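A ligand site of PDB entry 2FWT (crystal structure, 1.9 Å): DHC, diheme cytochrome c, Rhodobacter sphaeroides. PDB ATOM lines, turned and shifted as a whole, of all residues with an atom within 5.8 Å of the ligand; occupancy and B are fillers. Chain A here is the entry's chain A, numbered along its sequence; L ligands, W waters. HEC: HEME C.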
ATOM      1  N   TYR A  20      22.826 -19.082  -1.679  1.00  0.00           N
ATOM      2  CA  TYR A  20      22.341 -19.418  -3.021  1.00  0.00           C
ATOM      3  C   TYR A  20      21.236 -18.469  -3.463  1.00  0.00           C
ATOM      4  O   TYR A  20      20.283 -18.246  -2.725  1.00  0.00           O
ATOM      5  CB  TYR A  20      21.812 -20.841  -3.063  1.00  0.00           C
ATOM      6  CG  TYR A  20      22.855 -21.902  -2.742  1.00  0.00           C
ATOM      7  CD1 TYR A  20      22.765 -22.692  -1.602  1.00  0.00           C
ATOM      8  CD2 TYR A  20      23.929 -22.079  -3.558  1.00  0.00           C
ATOM      9  CE1 TYR A  20      23.727 -23.651  -1.319  1.00  0.00           C
ATOM     10  CE2 TYR A  20      24.920 -23.047  -3.285  1.00  0.00           C
ATOM     11  CZ  TYR A  20      24.810 -23.817  -2.170  1.00  0.00           C
ATOM     12  OH  TYR A  20      25.774 -24.760  -1.899  1.00  0.00           O
ATOM     13  N   LEU A  24      17.532 -19.568  -8.488  1.00  0.00           N
ATOM     14  CA  LEU A  24      18.041 -20.880  -8.901  1.00  0.00           C
ATOM     15  C   LEU A  24      17.095 -22.074  -8.644  1.00  0.00           C
ATOM     16  O   LEU A  24      17.268 -23.124  -9.273  1.00  0.00           O
ATOM     17  CB  LEU A  24      19.385 -21.141  -8.254  1.00  0.00           C
ATOM     18  CG  LEU A  24      20.714 -20.785  -8.954  1.00  0.00           C
ATOM     19  CD1 LEU A  24      20.671 -19.947 -10.209  1.00  0.00           C
ATOM     20  CD2 LEU A  24      21.787 -20.384  -8.003  1.00  0.00           C
ATOM     21  N   ILE A  85      19.997 -27.389  -6.153  1.00  0.00           N
ATOM     22  CA  ILE A  85      20.342 -26.766  -7.409  1.00  0.00           C
ATOM     23  C   ILE A  85      21.195 -27.747  -8.248  1.00  0.00           C
ATOM     24  O   ILE A  85      20.985 -27.893  -9.461  1.00  0.00           O
ATOM     25  CB  ILE A  85      21.122 -25.461  -7.183  1.00  0.00           C
ATOM     26  CG1 ILE A  85      20.250 -24.424  -6.421  1.00  0.00           C
ATOM     27  CG2 ILE A  85      21.589 -24.866  -8.514  1.00  0.00           C
ATOM     28  CD1 ILE A  85      21.073 -23.376  -5.684  1.00  0.00           C
ATOM     29  N   SER A  86      22.107 -28.422  -7.577  1.00  0.00           N
ATOM     30  CA  SER A  86      23.042 -29.358  -8.198  1.00  0.00           C
ATOM     31  C   SER A  86      22.385 -30.625  -8.761  1.00  0.00           C
ATOM     32  O   SER A  86      23.062 -31.422  -9.406  1.00  0.00           O
ATOM     33  CB  SER A  86      24.155 -29.717  -7.204  1.00  0.00           C
ATOM     34  OG  SER A  86      23.664 -30.462  -6.109  1.00  0.00           O
ATOM     35  N   TRP A  90      19.200 -28.837 -15.946  1.00  0.00           N
ATOM     36  CA  TRP A  90      20.219 -28.044 -16.645  1.00  0.00           C
ATOM     37  C   TRP A  90      21.585 -28.215 -15.994  1.00  0.00           C
ATOM     38  O   TRP A  90      22.620 -28.211 -16.674  1.00  0.00           O
ATOM     39  CB  TRP A  90      19.827 -26.566 -16.751  1.00  0.00           C
ATOM     40  CG  TRP A  90      19.830 -25.761 -15.465  1.00  0.00           C
ATOM     41  CD1 TRP A  90      18.755 -25.367 -14.760  1.00  0.00           C
ATOM     42  CD2 TRP A  90      20.969 -25.244 -14.786  1.00  0.00           C
ATOM     43  NE1 TRP A  90      19.163 -24.620 -13.646  1.00  0.00           N
ATOM     44  CE2 TRP A  90      20.517 -24.523 -13.656  1.00  0.00           C
ATOM     45  CE3 TRP A  90      22.342 -25.264 -15.051  1.00  0.00           C
ATOM     46  CZ2 TRP A  90      21.380 -23.907 -12.755  1.00  0.00           C
ATOM     47  CZ3 TRP A  90      23.205 -24.640 -14.156  1.00  0.00           C
ATOM     48  CH2 TRP A  90      22.706 -23.971 -13.031  1.00  0.00           C
ATOM     49  N   PHE A  91      21.589 -28.337 -14.674  1.00  0.00           N
ATOM     50  CA  PHE A  91      22.848 -28.364 -13.924  1.00  0.00           C
ATOM     51  C   PHE A  91      23.589 -29.640 -14.249  1.00  0.00           C
ATOM     52  O   PHE A  91      24.792 -29.636 -14.530  1.00  0.00           O
ATOM     53  CB  PHE A  91      22.552 -28.306 -12.426  1.00  0.00           C
ATOM     54  CG  PHE A  91      23.781 -28.124 -11.601  1.00  0.00           C
ATOM     55  CD1 PHE A  91      24.088 -26.895 -11.055  1.00  0.00           C
ATOM     56  CD2 PHE A  91      24.637 -29.194 -11.344  1.00  0.00           C
ATOM     57  CE1 PHE A  91      25.231 -26.738 -10.273  1.00  0.00           C
ATOM     58  CE2 PHE A  91      25.781 -29.034 -10.539  1.00  0.00           C
ATOM     59  CZ  PHE A  91      26.085 -27.822 -10.017  1.00  0.00           C
ATOM     60  N   LYS A  94      24.795 -29.559 -18.076  1.00  0.00           N
ATOM     61  CA  LYS A  94      25.907 -28.652 -18.347  1.00  0.00           C
ATOM     62  C   LYS A  94      27.205 -29.072 -17.650  1.00  0.00           C
ATOM     63  O   LYS A  94      28.288 -29.050 -18.252  1.00  0.00           O
ATOM     64  CB  LYS A  94      25.510 -27.208 -17.999  1.00  0.00           C
ATOM     65  CG  LYS A  94      24.378 -26.666 -18.851  1.00  0.00           C
ATOM     66  CD  LYS A  94      24.661 -26.595 -20.328  1.00  0.00           C
ATOM     67  CE  LYS A  94      23.548 -25.866 -21.082  1.00  0.00           C
ATOM     68  NZ  LYS A  94      23.820 -25.637 -22.550  1.00  0.00           N
ATOM     69  N   HIS A  95      27.133 -29.518 -16.417  1.00  0.00           N
ATOM     70  CA  HIS A  95      28.341 -29.849 -15.710  1.00  0.00           C
ATOM     71  C   HIS A  95      28.915 -31.203 -16.139  1.00  0.00           C
ATOM     72  O   HIS A  95      30.108 -31.449 -15.970  1.00  0.00           O
ATOM     73  CB  HIS A  95      28.090 -29.773 -14.184  1.00  0.00           C
ATOM     74  CG  HIS A  95      27.964 -28.360 -13.668  1.00  0.00           C
ATOM     75  ND1 HIS A  95      26.757 -27.699 -13.603  1.00  0.00           N
ATOM     76  CD2 HIS A  95      28.898 -27.477 -13.240  1.00  0.00           C
ATOM     77  CE1 HIS A  95      26.959 -26.467 -13.131  1.00  0.00           C
ATOM     78  NE2 HIS A  95      28.257 -26.284 -12.931  1.00  0.00           N
ATOM     79  N   GLU A  98      31.647 -30.470 -18.570  1.00  0.00           N
ATOM     80  CA  GLU A  98      32.623 -29.461 -18.204  1.00  0.00           C
ATOM     81  C   GLU A  98      33.435 -29.779 -16.968  1.00  0.00           C
ATOM     82  O   GLU A  98      34.453 -29.167 -16.741  1.00  0.00           O
ATOM     83  CB  GLU A  98      31.901 -28.128 -18.000  1.00  0.00           C
ATOM     84  CG  GLU A  98      31.296 -27.572 -19.283  1.00  0.00           C
ATOM     85  CD  GLU A  98      32.310 -27.075 -20.276  1.00  0.00           C
ATOM     86  OE1 GLU A  98      33.488 -26.875 -19.933  1.00  0.00           O
ATOM     87  OE2 GLU A  98      31.916 -26.854 -21.419  1.00  0.00           O
ATOM     88  N   VAL A  99      32.996 -30.747 -16.180  1.00  0.00           N
ATOM     89  CA  VAL A  99      33.632 -31.042 -14.895  1.00  0.00           C
ATOM     90  C   VAL A  99      34.268 -32.419 -14.966  1.00  0.00           C
ATOM     91  O   VAL A  99      33.561 -33.425 -15.087  1.00  0.00           O
ATOM     92  CB  VAL A  99      32.612 -31.029 -13.727  1.00  0.00           C
ATOM     93  CG1 VAL A  99      33.248 -31.487 -12.459  1.00  0.00           C
ATOM     94  CG2 VAL A  99      32.005 -29.642 -13.556  1.00  0.00           C
ATOM     95  N   MET A 103      38.288 -32.607 -11.006  1.00  0.00           N
ATOM     96  CA  MET A 103      37.727 -31.303 -10.592  1.00  0.00           C
ATOM     97  C   MET A 103      36.690 -31.472  -9.499  1.00  0.00           C
ATOM     98  O   MET A 103      36.668 -30.710  -8.505  1.00  0.00           O
ATOM     99  CB  MET A 103      37.113 -30.560 -11.761  1.00  0.00           C
ATOM    100  CG  MET A 103      38.117 -30.062 -12.753  1.00  0.00           C
ATOM    101  SD  MET A 103      37.337 -29.620 -14.338  1.00  0.00           S
ATOM    102  CE  MET A 103      36.255 -28.280 -13.793  1.00  0.00           C
ATOM    103  N   LEU A 104      35.839 -32.483  -9.657  1.00  0.00           N
ATOM    104  CA  LEU A 104      34.823 -32.766  -8.647  1.00  0.00           C
ATOM    105  C   LEU A 104      35.459 -33.243  -7.339  1.00  0.00           C
ATOM    106  O   LEU A 104      35.072 -32.793  -6.244  1.00  0.00           O
ATOM    107  CB  LEU A 104      33.822 -33.804  -9.187  1.00  0.00           C
ATOM    108  CG  LEU A 104      32.850 -34.390  -8.160  1.00  0.00           C
ATOM    109  CD1 LEU A 104      32.061 -33.267  -7.525  1.00  0.00           C
ATOM    110  CD2 LEU A 104      31.916 -35.390  -8.827  1.00  0.00           C
ATOM    111  N   ALA A 107      36.934 -30.141  -5.593  1.00  0.00           N
ATOM    112  CA  ALA A 107      35.919 -29.223  -5.085  1.00  0.00           C
ATOM    113  C   ALA A 107      35.135 -29.840  -3.914  1.00  0.00           C
ATOM    114  O   ALA A 107      34.390 -29.135  -3.215  1.00  0.00           O
ATOM    115  CB  ALA A 107      34.930 -28.837  -6.232  1.00  0.00           C
ATOM    116  N   SER A 109      32.366 -31.178  -3.488  1.00  0.00           N
ATOM    117  CA  SER A 109      30.926 -31.265  -3.724  1.00  0.00           C
ATOM    118  C   SER A 109      30.497 -30.284  -4.810  1.00  0.00           C
ATOM    119  O   SER A 109      30.995 -29.152  -4.874  1.00  0.00           O
ATOM    120  CB  SER A 109      30.133 -30.948  -2.428  1.00  0.00           C
ATOM    121  OG  SER A 109      28.736 -30.925  -2.664  1.00  0.00           O
ATOM    122  N   MET A 110      29.534 -30.689  -5.638  1.00  0.00           N
ATOM    123  CA  MET A 110      28.976 -29.749  -6.624  1.00  0.00           C
ATOM    124  C   MET A 110      28.212 -28.606  -5.944  1.00  0.00           C
ATOM    125  O   MET A 110      27.929 -27.590  -6.603  1.00  0.00           O
ATOM    126  CB  MET A 110      28.092 -30.483  -7.633  1.00  0.00           C
ATOM    127  CG  MET A 110      28.889 -31.398  -8.524  1.00  0.00           C
ATOM    128  SD  MET A 110      30.299 -30.627  -9.381  1.00  0.00           S
ATOM    129  CE  MET A 110      29.476 -29.379 -10.365  1.00  0.00           C
ATOM    130  N   SER A 111      27.899 -28.740  -4.654  1.00  0.00           N
ATOM    131  CA  SER A 111      27.288 -27.639  -3.881  1.00  0.00           C
ATOM    132  C   SER A 111      28.242 -26.457  -3.703  1.00  0.00           C
ATOM    133  O   SER A 111      27.780 -25.328  -3.463  1.00  0.00           O
ATOM    134  CB  SER A 111      26.858 -28.123  -2.500  1.00  0.00           C
ATOM    135  OG  SER A 111      26.044 -29.277  -2.595  1.00  0.00           O
ATOM    136  N   ASN A 112      29.548 -26.701  -3.803  1.00  0.00           N
ATOM    137  CA  ASN A 112      30.569 -25.684  -3.539  1.00  0.00           C
ATOM    138  C   ASN A 112      30.882 -24.841  -4.754  1.00  0.00           C
ATOM    139  O   ASN A 112      31.955 -24.983  -5.357  1.00  0.00           O
ATOM    140  CB  ASN A 112      31.829 -26.389  -3.040  1.00  0.00           C
ATOM    141  CG  ASN A 112      32.917 -25.444  -2.532  1.00  0.00           C
ATOM    142  OD1 ASN A 112      32.748 -24.184  -2.373  1.00  0.00           O
ATOM    143  ND2 ASN A 112      34.083 -26.053  -2.264  1.00  0.00           N
ATOM    144  N   CYS A 113      29.906 -24.005  -5.169  1.00  0.00           N
ATOM    145  CA  CYS A 113      30.030 -23.290  -6.421  1.00  0.00           C
ATOM    146  C   CYS A 113      31.313 -22.487  -6.516  1.00  0.00           C
ATOM    147  O   CYS A 113      31.937 -22.411  -7.588  1.00  0.00           O
ATOM    148  CB  CYS A 113      28.849 -22.381  -6.708  1.00  0.00           C
ATOM    149  SG  CYS A 113      27.247 -22.961  -6.214  1.00  0.00           S
ATOM    150  N   ALA A 115      34.260 -22.965  -5.373  1.00  0.00           N
ATOM    151  CA  ALA A 115      35.493 -23.744  -5.592  1.00  0.00           C
ATOM    152  C   ALA A 115      35.885 -23.767  -7.067  1.00  0.00           C
ATOM    153  O   ALA A 115      37.070 -23.958  -7.426  1.00  0.00           O
ATOM    154  CB  ALA A 115      35.306 -25.126  -5.114  1.00  0.00           C
ATOM    155  N   CYS A 116      34.897 -23.530  -7.928  1.00  0.00           N
ATOM    156  CA  CYS A 116      35.116 -23.507  -9.360  1.00  0.00           C
ATOM    157  C   CYS A 116      34.775 -22.216 -10.025  1.00  0.00           C
ATOM    158  O   CYS A 116      35.357 -21.906 -11.074  1.00  0.00           O
ATOM    159  CB  CYS A 116      34.303 -24.614  -9.992  1.00  0.00           C
ATOM    160  SG  CYS A 116      34.813 -26.221  -9.396  1.00  0.00           S
ATOM    161  N   HIS A 117      33.800 -21.479  -9.489  1.00  0.00           N
ATOM    162  CA  HIS A 117      33.324 -20.244 -10.091  1.00  0.00           C
ATOM    163  C   HIS A 117      33.827 -19.059  -9.268  1.00  0.00           C
ATOM    164  O   HIS A 117      33.290 -18.749  -8.208  1.00  0.00           O
ATOM    165  CB  HIS A 117      31.786 -20.232 -10.171  1.00  0.00           C
ATOM    166  CG  HIS A 117      31.214 -21.257 -11.103  1.00  0.00           C
ATOM    167  ND1 HIS A 117      31.233 -21.095 -12.468  1.00  0.00           N
ATOM    168  CD2 HIS A 117      30.542 -22.426 -10.870  1.00  0.00           C
ATOM    169  CE1 HIS A 117      30.642 -22.147 -13.038  1.00  0.00           C
ATOM    170  NE2 HIS A 117      30.193 -22.956 -12.091  1.00  0.00           N
ATOM    171  N   PHE A 125      28.711 -16.893 -13.153  1.00  0.00           N
ATOM    172  CA  PHE A 125      29.011 -18.314 -13.314  1.00  0.00           C
ATOM    173  C   PHE A 125      29.561 -18.577 -14.711  1.00  0.00           C
ATOM    174  O   PHE A 125      29.864 -17.593 -15.439  1.00  0.00           O
ATOM    175  CB  PHE A 125      27.739 -19.119 -13.055  1.00  0.00           C
ATOM    176  CG  PHE A 125      27.179 -18.933 -11.662  1.00  0.00           C
ATOM    177  CD1 PHE A 125      26.212 -17.979 -11.401  1.00  0.00           C
ATOM    178  CD2 PHE A 125      27.637 -19.732 -10.615  1.00  0.00           C
ATOM    179  CE1 PHE A 125      25.713 -17.812 -10.128  1.00  0.00           C
ATOM    180  CE2 PHE A 125      27.135 -19.579  -9.344  1.00  0.00           C
ATOM    181  CZ  PHE A 125      26.179 -18.626  -9.084  1.00  0.00           C
HETATM  182 FE   HEC L   1      29.180 -24.619 -12.430  1.00  0.00          FE
HETATM  183  CHA HEC L   1      29.045 -23.971 -15.763  1.00  0.00           C
HETATM  184  CHB HEC L   1      26.397 -22.729 -11.899  1.00  0.00           C
HETATM  185  CHC HEC L   1      29.131 -25.584  -9.171  1.00  0.00           C
HETATM  186  CHD HEC L   1      32.267 -26.009 -12.802  1.00  0.00           C
HETATM  187  NA  HEC L   1      27.948 -23.554 -13.614  1.00  0.00           N
HETATM  188  C1A HEC L   1      28.031 -23.445 -14.976  1.00  0.00           C
HETATM  189  C2A HEC L   1      26.956 -22.646 -15.449  1.00  0.00           C
HETATM  190  C3A HEC L   1      26.225 -22.276 -14.378  1.00  0.00           C
HETATM  191  C4A HEC L   1      26.840 -22.848 -13.198  1.00  0.00           C
HETATM  192  CMA HEC L   1      24.978 -21.387 -14.414  1.00  0.00           C
HETATM  193  CAA HEC L   1      26.660 -22.269 -16.925  1.00  0.00           C
HETATM  194  CBA HEC L   1      25.627 -23.248 -17.441  1.00  0.00           C
HETATM  195  CGA HEC L   1      25.337 -23.063 -18.938  1.00  0.00           C
HETATM  196  O1A HEC L   1      24.196 -22.715 -19.266  1.00  0.00           O
HETATM  197  O2A HEC L   1      26.226 -23.238 -19.802  1.00  0.00           O
HETATM  198  NB  HEC L   1      28.002 -24.236 -10.834  1.00  0.00           N
HETATM  199  C1B HEC L   1      26.880 -23.420 -10.822  1.00  0.00           C
HETATM  200  C2B HEC L   1      26.303 -23.415  -9.505  1.00  0.00           C
HETATM  201  C3B HEC L   1      27.055 -24.220  -8.738  1.00  0.00           C
HETATM  202  C4B HEC L   1      28.137 -24.735  -9.569  1.00  0.00           C
HETATM  203  CMB HEC L   1      25.039 -22.636  -9.156  1.00  0.00           C
HETATM  204  CAB HEC L   1      26.843 -24.618  -7.255  1.00  0.00           C
HETATM  205  CBB HEC L   1      25.585 -25.065  -6.851  1.00  0.00           C
HETATM  206  NC  HEC L   1      30.474 -25.600 -11.229  1.00  0.00           N
HETATM  207  C1C HEC L   1      30.242 -25.923  -9.899  1.00  0.00           C
HETATM  208  C2C HEC L   1      31.384 -26.673  -9.422  1.00  0.00           C
HETATM  209  C3C HEC L   1      32.270 -26.808 -10.416  1.00  0.00           C
HETATM  210  C4C HEC L   1      31.711 -26.118 -11.567  1.00  0.00           C
HETATM  211  CMC HEC L   1      31.487 -27.198  -7.995  1.00  0.00           C
HETATM  212  CAC HEC L   1      33.635 -27.552 -10.393  1.00  0.00           C
HETATM  213  CBC HEC L   1      33.772 -28.762  -9.756  1.00  0.00           C
HETATM  214  ND  HEC L   1      30.411 -24.937 -13.969  1.00  0.00           N
HETATM  215  C1D HEC L   1      31.680 -25.497 -13.893  1.00  0.00           C
HETATM  216  C2D HEC L   1      32.339 -25.421 -15.195  1.00  0.00           C
HETATM  217  C3D HEC L   1      31.364 -24.786 -16.127  1.00  0.00           C
HETATM  218  C4D HEC L   1      30.189 -24.534 -15.287  1.00  0.00           C
HETATM  219  CMD HEC L   1      33.742 -25.894 -15.542  1.00  0.00           C
HETATM  220  CAD HEC L   1      31.543 -24.475 -17.628  1.00  0.00           C
HETATM  221  CBD HEC L   1      32.011 -23.019 -17.815  1.00  0.00           C
HETATM  222  CGD HEC L   1      31.660 -22.482 -19.200  1.00  0.00           C
HETATM  223  O1D HEC L   1      31.253 -23.214 -20.161  1.00  0.00           O
HETATM  224  O2D HEC L   1      31.748 -21.244 -19.379  1.00  0.00           O
HETATM  225  O   HOH W   1      24.490 -21.036 -21.537  1.00  0.00           O
HETATM  226  O   HOH W   2      26.120 -23.906 -22.565  1.00  0.00           O
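An iron atom (FE) of the ligand is bound by a ring nitrogen (NE2) of His 95 (2.0 Å).
NE2 of His 117 binds FE of the ligand (2.0 Å).
A carbon (CAB) of the ligand is bonded to the side-chain sulfur (SG) of Cys 113.
A carbon (CAC) of the ligand is covalently linked to the side-chain sulfur of Cys 116 (2.0 Å).
A ring nitrogen (ND1) of His 95 is in hydrogen-bond range of the backbone carbonyl oxygen of Phe 91, 2.9 Å away.
The side-chain amide nitrogen (ND2) of Asn 112 sits at hydrogen-bond distance from the backbone carbonyl oxygen (O) of Ala 107.
The backbone NH of Ser 111 sits close to the side-chain hydroxyl of Ser 109 (3.1 Å).
The backbone carbonyl oxygen of Ser 111 sits at hydrogen-bond distance from the side-chain hydroxyl of Tyr 20 (2.6 Å).
CH2 of Trp 90 touches CMA of the ligand, at 3.7 Å.
CE1 of Phe 91 touches C3B of the ligand, at 3.5 Å.
Lys 94 touches the ligand (CE to O1A, 3.7 Å).
Glu 98 touches the ligand (CG to CAD, 3.5 Å).
Val 99 touches the ligand (CG2 to CHD, 3.7 Å).
O of Met 103 touches CBC of the ligand, at 3.7 Å.
Ala 107 touches the ligand.
O of Ser 109 touches CMC of the ligand, at 3.7 Å.
Met 110 touches the ligand.
Ser 111 touches the ligand.
Asn 112 touches the ligand.
Phe 125 touches the ligand.
Hydrophobic or aromatic side chains within 4 Å of the ligand: Trp 90, Phe 91, His 95, Val 99, Met 103, Ala 107, Met 110, His 117 and Phe 125.
Within 4 Å of the ligand: Trp 90, Phe 91, Lys 94, His 95, Glu 98, Val 99, Met 103, Ala 107, Ser 109, Met 110, Ser 111, Asn 112, Cys 113, Cys 116, His 117 and Phe 125.
Water W2 lies within hydrogen-bond range of an oxygen (O2A) of the ligand (2.8 Å) and the side-chain amino group (NZ) of Lys 94 (2.9 Å).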
